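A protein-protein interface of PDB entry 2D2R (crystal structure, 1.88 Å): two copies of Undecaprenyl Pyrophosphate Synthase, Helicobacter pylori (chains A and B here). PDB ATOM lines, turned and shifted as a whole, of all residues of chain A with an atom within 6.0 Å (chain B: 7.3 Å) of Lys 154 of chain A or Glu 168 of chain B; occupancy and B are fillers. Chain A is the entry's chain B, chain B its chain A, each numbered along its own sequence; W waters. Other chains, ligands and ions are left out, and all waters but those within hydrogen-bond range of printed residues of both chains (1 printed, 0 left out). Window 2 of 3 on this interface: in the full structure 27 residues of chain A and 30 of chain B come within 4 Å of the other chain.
Among the printed residues, pairs that only touch across the chains: Ser 150 of chain A with Ser 169 of chain B (3.6 Å), Ser 150 of chain A with Glu 171 of chain B (3.9 Å), Phe 153 of chain A with Phe 153 of chain B (3.6 Å), Phe 153 of chain A with Ile 174 of chain B (3.4 Å), Lys 154 of chain A with Leu 167 of chain B (3.5 Å), Lys 154 of chain A with Leu 170 of chain B (3.8 Å), Leu 156 of chain A with Phe 153 of chain B (3.3 Å) and Leu 157 of chain A with Phe 153 of chain B (3.7 Å).
Water W1 lies within hydrogen-bond range of O of Glu 168 of chain B (2.8 Å) and OG of Ser 150 of chain A (2.9 Å).
Lys 154 of chain A touches three residues of chain B. Glu 158 of chain A touches none of the printed residues of chain B. Printed residues of chain A within 4 Å of Phe 153 of chain B: Phe 153 (3.6 Å), Leu 156 (3.3 Å) and Leu 157 (3.7 Å). Of chain A, only Lys 154 (3.3 Å) comes within 4 Å of Glu 168 of chain B. Of the printed residues of chain A, Ser 169 of chain B touches Ser 150. The nearest residue of chain B that does not touch Lys 154 of chain A is Ile 164 of chain B (4.8 Å). The nearest residue of chain A that does not touch Glu 168 of chain B is Ser 150 of chain A (4.2 Å). The nearest printed residue of chain A that does not touch Ser 169 of chain B is Lys 154 of chain A (6.0 Å).
Hydrophobic or aromatic side chains of chain B within 4 Å of the printed part of chain A: Phe 153, Leu 170 and Ile 174. Along chain B the printed residues that touch a printed residue of chain A span positions 153 to 174. Hydrophobic or aromatic side chains of chain A that line the printed part of chain B: Phe 153, Leu 156 and Leu 157. Among the printed residues, 10 pairs touch across the chains.
Phe 153 of chain B touches its own counterpart, Phe 153 of chain A. Of the 10 pairs that touch across the chains among the printed residues, 1 has its exchanged pair printed and touching as well.
OE1 of Glu 168 of chain B is in salt-bridge range of NZ of Lys 154 of chain A (3.3 Å). The backbone NH (N) of Leu 170 of chain B lies within hydrogen-bond range of the side-chain hydroxyl (OG) of Ser 150 of chain A (2.7 Å).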
ATOM      1  N   LEU A 149     -21.187  12.482 -16.835  1.00  0.00           N
ATOM      2  CA  LEU A 149     -22.079  12.482 -15.643  1.00  0.00           C
ATOM      3  C   LEU A 149     -22.647  13.923 -15.390  1.00  0.00           C
ATOM      4  O   LEU A 149     -23.820  14.095 -15.041  1.00  0.00           O
ATOM      5  CB  LEU A 149     -21.274  11.969 -14.447  1.00  0.00           C
ATOM      6  CG  LEU A 149     -21.157  10.425 -14.418  1.00  0.00           C
ATOM      7  CD1 LEU A 149     -20.127  10.014 -13.447  1.00  0.00           C
ATOM      8  CD2 LEU A 149     -22.543   9.811 -13.970  1.00  0.00           C
ATOM      9  N   SER A 150     -21.823  14.934 -15.654  1.00  0.00           N
ATOM     10  CA  SER A 150     -22.272  16.309 -15.514  1.00  0.00           C
ATOM     11  C   SER A 150     -23.462  16.595 -16.418  1.00  0.00           C
ATOM     12  O   SER A 150     -24.455  17.183 -15.959  1.00  0.00           O
ATOM     13  CB  SER A 150     -21.134  17.302 -15.850  1.00  0.00           C
ATOM     14  OG  SER A 150     -21.637  18.633 -15.889  1.00  0.00           O
ATOM     15  N   ARG A 151     -23.368  16.163 -17.685  1.00  0.00           N
ATOM     16  CA  ARG A 151     -24.401  16.384 -18.668  1.00  0.00           C
ATOM     17  C   ARG A 151     -25.610  15.564 -18.311  1.00  0.00           C
ATOM     18  O   ARG A 151     -26.752  16.024 -18.461  1.00  0.00           O
ATOM     19  CB  ARG A 151     -23.901  16.036 -20.102  1.00  0.00           C
ATOM     20  CG  ARG A 151     -22.900  17.067 -20.609  1.00  0.00           C
ATOM     21  CD  ARG A 151     -22.397  16.799 -22.078  1.00  0.00           C
ATOM     22  NE  ARG A 151     -21.473  15.648 -22.148  1.00  0.00           N
ATOM     23  CZ  ARG A 151     -21.782  14.446 -22.670  1.00  0.00           C
ATOM     24  NH1 ARG A 151     -22.998  14.211 -23.168  1.00  0.00           N
ATOM     25  NH2 ARG A 151     -20.860  13.477 -22.676  1.00  0.00           N
ATOM     26  N   ALA A 152     -25.393  14.362 -17.772  1.00  0.00           N
ATOM     27  CA  ALA A 152     -26.550  13.559 -17.419  1.00  0.00           C
ATOM     28  C   ALA A 152     -27.247  14.224 -16.211  1.00  0.00           C
ATOM     29  O   ALA A 152     -28.468  14.268 -16.148  1.00  0.00           O
ATOM     30  CB  ALA A 152     -26.112  12.112 -17.066  1.00  0.00           C
ATOM     31  N   PHE A 153     -26.474  14.664 -15.223  1.00  0.00           N
ATOM     32  CA  PHE A 153     -27.048  15.342 -14.060  1.00  0.00           C
ATOM     33  C   PHE A 153     -27.824  16.611 -14.440  1.00  0.00           C
ATOM     34  O   PHE A 153     -28.900  16.868 -13.893  1.00  0.00           O
ATOM     35  CB  PHE A 153     -25.960  15.732 -13.083  1.00  0.00           C
ATOM     36  CG  PHE A 153     -25.593  14.629 -12.130  1.00  0.00           C
ATOM     37  CD1 PHE A 153     -25.593  13.307 -12.558  1.00  0.00           C
ATOM     38  CD2 PHE A 153     -25.183  14.918 -10.817  1.00  0.00           C
ATOM     39  CE1 PHE A 153     -25.167  12.265 -11.676  1.00  0.00           C
ATOM     40  CE2 PHE A 153     -24.765  13.918  -9.955  1.00  0.00           C
ATOM     41  CZ  PHE A 153     -24.752  12.581 -10.372  1.00  0.00           C
ATOM     42  N   LYS A 154     -27.257  17.408 -15.356  1.00  0.00           N
ATOM     43  CA  LYS A 154     -27.866  18.660 -15.782  1.00  0.00           C
ATOM     44  C   LYS A 154     -29.194  18.332 -16.421  1.00  0.00           C
ATOM     45  O   LYS A 154     -30.239  18.975 -16.159  1.00  0.00           O
ATOM     46  CB  LYS A 154     -26.902  19.396 -16.737  1.00  0.00           C
ATOM     47  CG  LYS A 154     -27.322  20.797 -17.174  1.00  0.00           C
ATOM     48  CD  LYS A 154     -27.269  21.837 -16.038  1.00  0.00           C
ATOM     49  CE  LYS A 154     -27.832  23.213 -16.508  1.00  0.00           C
ATOM     50  NZ  LYS A 154     -27.675  23.351 -18.004  1.00  0.00           N
ATOM     51  N   SER A 155     -29.173  17.299 -17.244  1.00  0.00           N
ATOM     52  CA  SER A 155     -30.365  16.843 -17.906  1.00  0.00           C
ATOM     53  C   SER A 155     -31.499  16.464 -16.930  1.00  0.00           C
ATOM     54  O   SER A 155     -32.651  16.832 -17.139  1.00  0.00           O
ATOM     55  CB  SER A 155     -30.027  15.634 -18.756  1.00  0.00           C
ATOM     56  OG  SER A 155     -31.208  15.053 -19.246  1.00  0.00           O
ATOM     57  N   LEU A 156     -31.163  15.689 -15.909  1.00  0.00           N
ATOM     58  CA  LEU A 156     -32.118  15.247 -14.891  1.00  0.00           C
ATOM     59  C   LEU A 156     -32.611  16.381 -13.993  1.00  0.00           C
ATOM     60  O   LEU A 156     -33.730  16.329 -13.495  1.00  0.00           O
ATOM     61  CB  LEU A 156     -31.473  14.200 -13.988  1.00  0.00           C
ATOM     62  CG  LEU A 156     -31.212  12.776 -14.496  1.00  0.00           C
ATOM     63  CD1 LEU A 156     -30.285  12.022 -13.525  1.00  0.00           C
ATOM     64  CD2 LEU A 156     -32.536  12.045 -14.646  1.00  0.00           C
ATOM     65  N   LEU A 157     -31.765  17.377 -13.754  1.00  0.00           N
ATOM     66  CA  LEU A 157     -32.135  18.483 -12.902  1.00  0.00           C
ATOM     67  C   LEU A 157     -33.126  19.302 -13.640  1.00  0.00           C
ATOM     68  O   LEU A 157     -34.113  19.765 -13.099  1.00  0.00           O
ATOM     69  CB  LEU A 157     -30.954  19.389 -12.597  1.00  0.00           C
ATOM     70  CG  LEU A 157     -29.954  19.010 -11.514  1.00  0.00           C
ATOM     71  CD1 LEU A 157     -29.028  20.200 -11.341  1.00  0.00           C
ATOM     72  CD2 LEU A 157     -30.655  18.668 -10.195  1.00  0.00           C
ATOM     73  N   GLU A 158     -32.824  19.502 -14.902  1.00  0.00           N
ATOM     74  CA  GLU A 158     -33.678  20.276 -15.744  1.00  0.00           C
ATOM     75  C   GLU A 158     -35.023  19.555 -15.910  1.00  0.00           C
ATOM     76  O   GLU A 158     -36.082  20.166 -15.770  1.00  0.00           O
ATOM     77  CB  GLU A 158     -32.940  20.503 -17.051  1.00  0.00           C
ATOM     78  CG  GLU A 158     -33.780  20.902 -18.193  1.00  0.00           C
ATOM     79  CD  GLU A 158     -33.009  20.763 -19.490  1.00  0.00           C
ATOM     80  OE1 GLU A 158     -32.063  21.566 -19.692  1.00  0.00           O
ATOM     81  OE2 GLU A 158     -33.337  19.843 -20.291  1.00  0.00           O
ATOM     82  N   SER A 159     -34.992  18.257 -16.180  1.00  0.00           N
ATOM     83  CA  SER A 159     -36.224  17.488 -16.335  1.00  0.00           C
ATOM     84  C   SER A 159     -36.185  16.272 -15.461  1.00  0.00           C
ATOM     85  O   SER A 159     -35.766  15.205 -15.897  1.00  0.00           O
ATOM     86  CB  SER A 159     -36.392  17.037 -17.764  1.00  0.00           C
ATOM     87  OG  SER A 159     -36.679  18.155 -18.559  1.00  0.00           O
ATOM     88  N   PHE B 153     -26.617  13.705  -6.464  1.00  0.00           N
ATOM     89  CA  PHE B 153     -27.593  14.278  -7.400  1.00  0.00           C
ATOM     90  C   PHE B 153     -28.854  14.743  -6.685  1.00  0.00           C
ATOM     91  O   PHE B 153     -29.442  15.784  -7.025  1.00  0.00           O
ATOM     92  CB  PHE B 153     -28.020  13.274  -8.470  1.00  0.00           C
ATOM     93  CG  PHE B 153     -29.227  13.727  -9.250  1.00  0.00           C
ATOM     94  CD1 PHE B 153     -29.094  14.603 -10.348  1.00  0.00           C
ATOM     95  CD2 PHE B 153     -30.504  13.323  -8.869  1.00  0.00           C
ATOM     96  CE1 PHE B 153     -30.240  15.069 -11.057  1.00  0.00           C
ATOM     97  CE2 PHE B 153     -31.655  13.773  -9.559  1.00  0.00           C
ATOM     98  CZ  PHE B 153     -31.531  14.653 -10.664  1.00  0.00           C
ATOM     99  N   ASN B 163     -26.929  29.838  -7.833  1.00  0.00           N
ATOM    100  CA  ASN B 163     -26.738  30.252  -9.250  1.00  0.00           C
ATOM    101  C   ASN B 163     -26.871  29.113 -10.257  1.00  0.00           C
ATOM    102  O   ASN B 163     -26.363  29.203 -11.425  1.00  0.00           O
ATOM    103  CB  ASN B 163     -25.375  30.909  -9.484  1.00  0.00           C
ATOM    104  CG  ASN B 163     -24.181  29.987  -9.212  1.00  0.00           C
ATOM    105  OD1 ASN B 163     -24.313  28.802  -8.738  1.00  0.00           O
ATOM    106  ND2 ASN B 163     -23.002  30.535  -9.417  1.00  0.00           N
ATOM    107  N   ILE B 164     -27.532  28.038  -9.832  1.00  0.00           N
ATOM    108  CA  ILE B 164     -27.655  26.908 -10.719  1.00  0.00           C
ATOM    109  C   ILE B 164     -28.062  27.299 -12.121  1.00  0.00           C
ATOM    110  O   ILE B 164     -27.708  26.634 -13.087  1.00  0.00           O
ATOM    111  CB  ILE B 164     -28.686  25.880 -10.209  1.00  0.00           C
ATOM    112  CG1 ILE B 164     -28.823  24.738 -11.216  1.00  0.00           C
ATOM    113  CG2 ILE B 164     -30.012  26.535 -10.029  1.00  0.00           C
ATOM    114  CD1 ILE B 164     -27.526  23.953 -11.428  1.00  0.00           C
ATOM    115  N   SER B 165     -28.798  28.393 -12.232  1.00  0.00           N
ATOM    116  CA  SER B 165     -29.302  28.863 -13.511  1.00  0.00           C
ATOM    117  C   SER B 165     -28.225  29.292 -14.513  1.00  0.00           C
ATOM    118  O   SER B 165     -28.417  29.249 -15.725  1.00  0.00           O
ATOM    119  CB  SER B 165     -30.181  30.087 -13.227  1.00  0.00           C
ATOM    120  OG  SER B 165     -31.213  30.179 -14.177  1.00  0.00           O
ATOM    121  N   LEU B 166     -27.136  29.803 -13.967  1.00  0.00           N
ATOM    122  CA  LEU B 166     -26.005  30.336 -14.748  1.00  0.00           C
ATOM    123  C   LEU B 166     -24.929  29.274 -14.980  1.00  0.00           C
ATOM    124  O   LEU B 166     -23.821  29.584 -15.453  1.00  0.00           O
ATOM    125  CB  LEU B 166     -25.365  31.507 -13.962  1.00  0.00           C
ATOM    126  CG  LEU B 166     -25.990  32.915 -13.922  1.00  0.00           C
ATOM    127  CD1 LEU B 166     -27.464  32.853 -14.177  1.00  0.00           C
ATOM    128  CD2 LEU B 166     -25.653  33.578 -12.565  1.00  0.00           C
ATOM    129  N   LEU B 167     -25.235  28.027 -14.655  1.00  0.00           N
ATOM    130  CA  LEU B 167     -24.242  27.000 -14.804  1.00  0.00           C
ATOM    131  C   LEU B 167     -24.459  26.088 -16.009  1.00  0.00           C
ATOM    132  O   LEU B 167     -25.566  25.938 -16.494  1.00  0.00           O
ATOM    133  CB  LEU B 167     -24.220  26.151 -13.526  1.00  0.00           C
ATOM    134  CG  LEU B 167     -23.985  26.783 -12.137  1.00  0.00           C
ATOM    135  CD1 LEU B 167     -23.852  25.681 -11.131  1.00  0.00           C
ATOM    136  CD2 LEU B 167     -22.713  27.657 -12.103  1.00  0.00           C
ATOM    137  N   GLU B 168     -23.399  25.475 -16.493  1.00  0.00           N
ATOM    138  CA  GLU B 168     -23.586  24.535 -17.561  1.00  0.00           C
ATOM    139  C   GLU B 168     -22.839  23.273 -17.099  1.00  0.00           C
ATOM    140  O   GLU B 168     -23.443  22.257 -16.884  1.00  0.00           O
ATOM    141  CB  GLU B 168     -23.066  25.080 -18.884  1.00  0.00           C
ATOM    142  CG  GLU B 168     -23.205  24.087 -20.015  1.00  0.00           C
ATOM    143  CD  GLU B 168     -24.642  23.712 -20.227  1.00  0.00           C
ATOM    144  OE1 GLU B 168     -25.525  24.624 -20.209  1.00  0.00           O
ATOM    145  OE2 GLU B 168     -24.882  22.504 -20.410  1.00  0.00           O
ATOM    146  N   SER B 169     -21.535  23.349 -16.926  1.00  0.00           N
ATOM    147  CA  SER B 169     -20.789  22.182 -16.426  1.00  0.00           C
ATOM    148  C   SER B 169     -21.049  22.099 -14.911  1.00  0.00           C
ATOM    149  O   SER B 169     -20.967  23.131 -14.211  1.00  0.00           O
ATOM    150  CB  SER B 169     -19.286  22.378 -16.727  1.00  0.00           C
ATOM    151  OG  SER B 169     -18.463  21.425 -16.065  1.00  0.00           O
ATOM    152  N   LEU B 170     -21.408  20.905 -14.409  1.00  0.00           N
ATOM    153  CA  LEU B 170     -21.648  20.708 -12.965  1.00  0.00           C
ATOM    154  C   LEU B 170     -20.599  19.910 -12.196  1.00  0.00           C
ATOM    155  O   LEU B 170     -20.805  19.547 -11.016  1.00  0.00           O
ATOM    156  CB  LEU B 170     -22.970  20.014 -12.769  1.00  0.00           C
ATOM    157  CG  LEU B 170     -24.158  20.720 -13.338  1.00  0.00           C
ATOM    158  CD1 LEU B 170     -25.379  19.854 -13.197  1.00  0.00           C
ATOM    159  CD2 LEU B 170     -24.313  22.068 -12.606  1.00  0.00           C
ATOM    160  N   GLU B 171     -19.470  19.602 -12.843  1.00  0.00           N
ATOM    161  CA  GLU B 171     -18.424  18.825 -12.169  1.00  0.00           C
ATOM    162  C   GLU B 171     -18.009  19.354 -10.802  1.00  0.00           C
ATOM    163  O   GLU B 171     -17.967  18.633  -9.810  1.00  0.00           O
ATOM    164  CB  GLU B 171     -17.140  18.660 -13.036  1.00  0.00           C
ATOM    165  CG  GLU B 171     -17.323  18.087 -14.430  1.00  0.00           C
ATOM    166  CD  GLU B 171     -15.995  17.822 -15.166  1.00  0.00           C
ATOM    167  OE1 GLU B 171     -16.038  17.749 -16.407  1.00  0.00           O
ATOM    168  OE2 GLU B 171     -14.914  17.676 -14.511  1.00  0.00           O
ATOM    169  N   ILE B 174     -20.712  18.692  -8.392  1.00  0.00           N
ATOM    170  CA  ILE B 174     -20.911  17.310  -7.962  1.00  0.00           C
ATOM    171  C   ILE B 174     -19.829  16.989  -6.986  1.00  0.00           C
ATOM    172  O   ILE B 174     -20.088  16.468  -5.903  1.00  0.00           O
ATOM    173  CB  ILE B 174     -20.850  16.369  -9.161  1.00  0.00           C
ATOM    174  CG1 ILE B 174     -22.070  16.595 -10.042  1.00  0.00           C
ATOM    175  CG2 ILE B 174     -20.752  14.901  -8.703  1.00  0.00           C
ATOM    176  CD1 ILE B 174     -22.020  15.849 -11.454  1.00  0.00           C
HETATM  177  O   HOH W   1     -22.980  19.844 -18.170  1.00  0.00           O
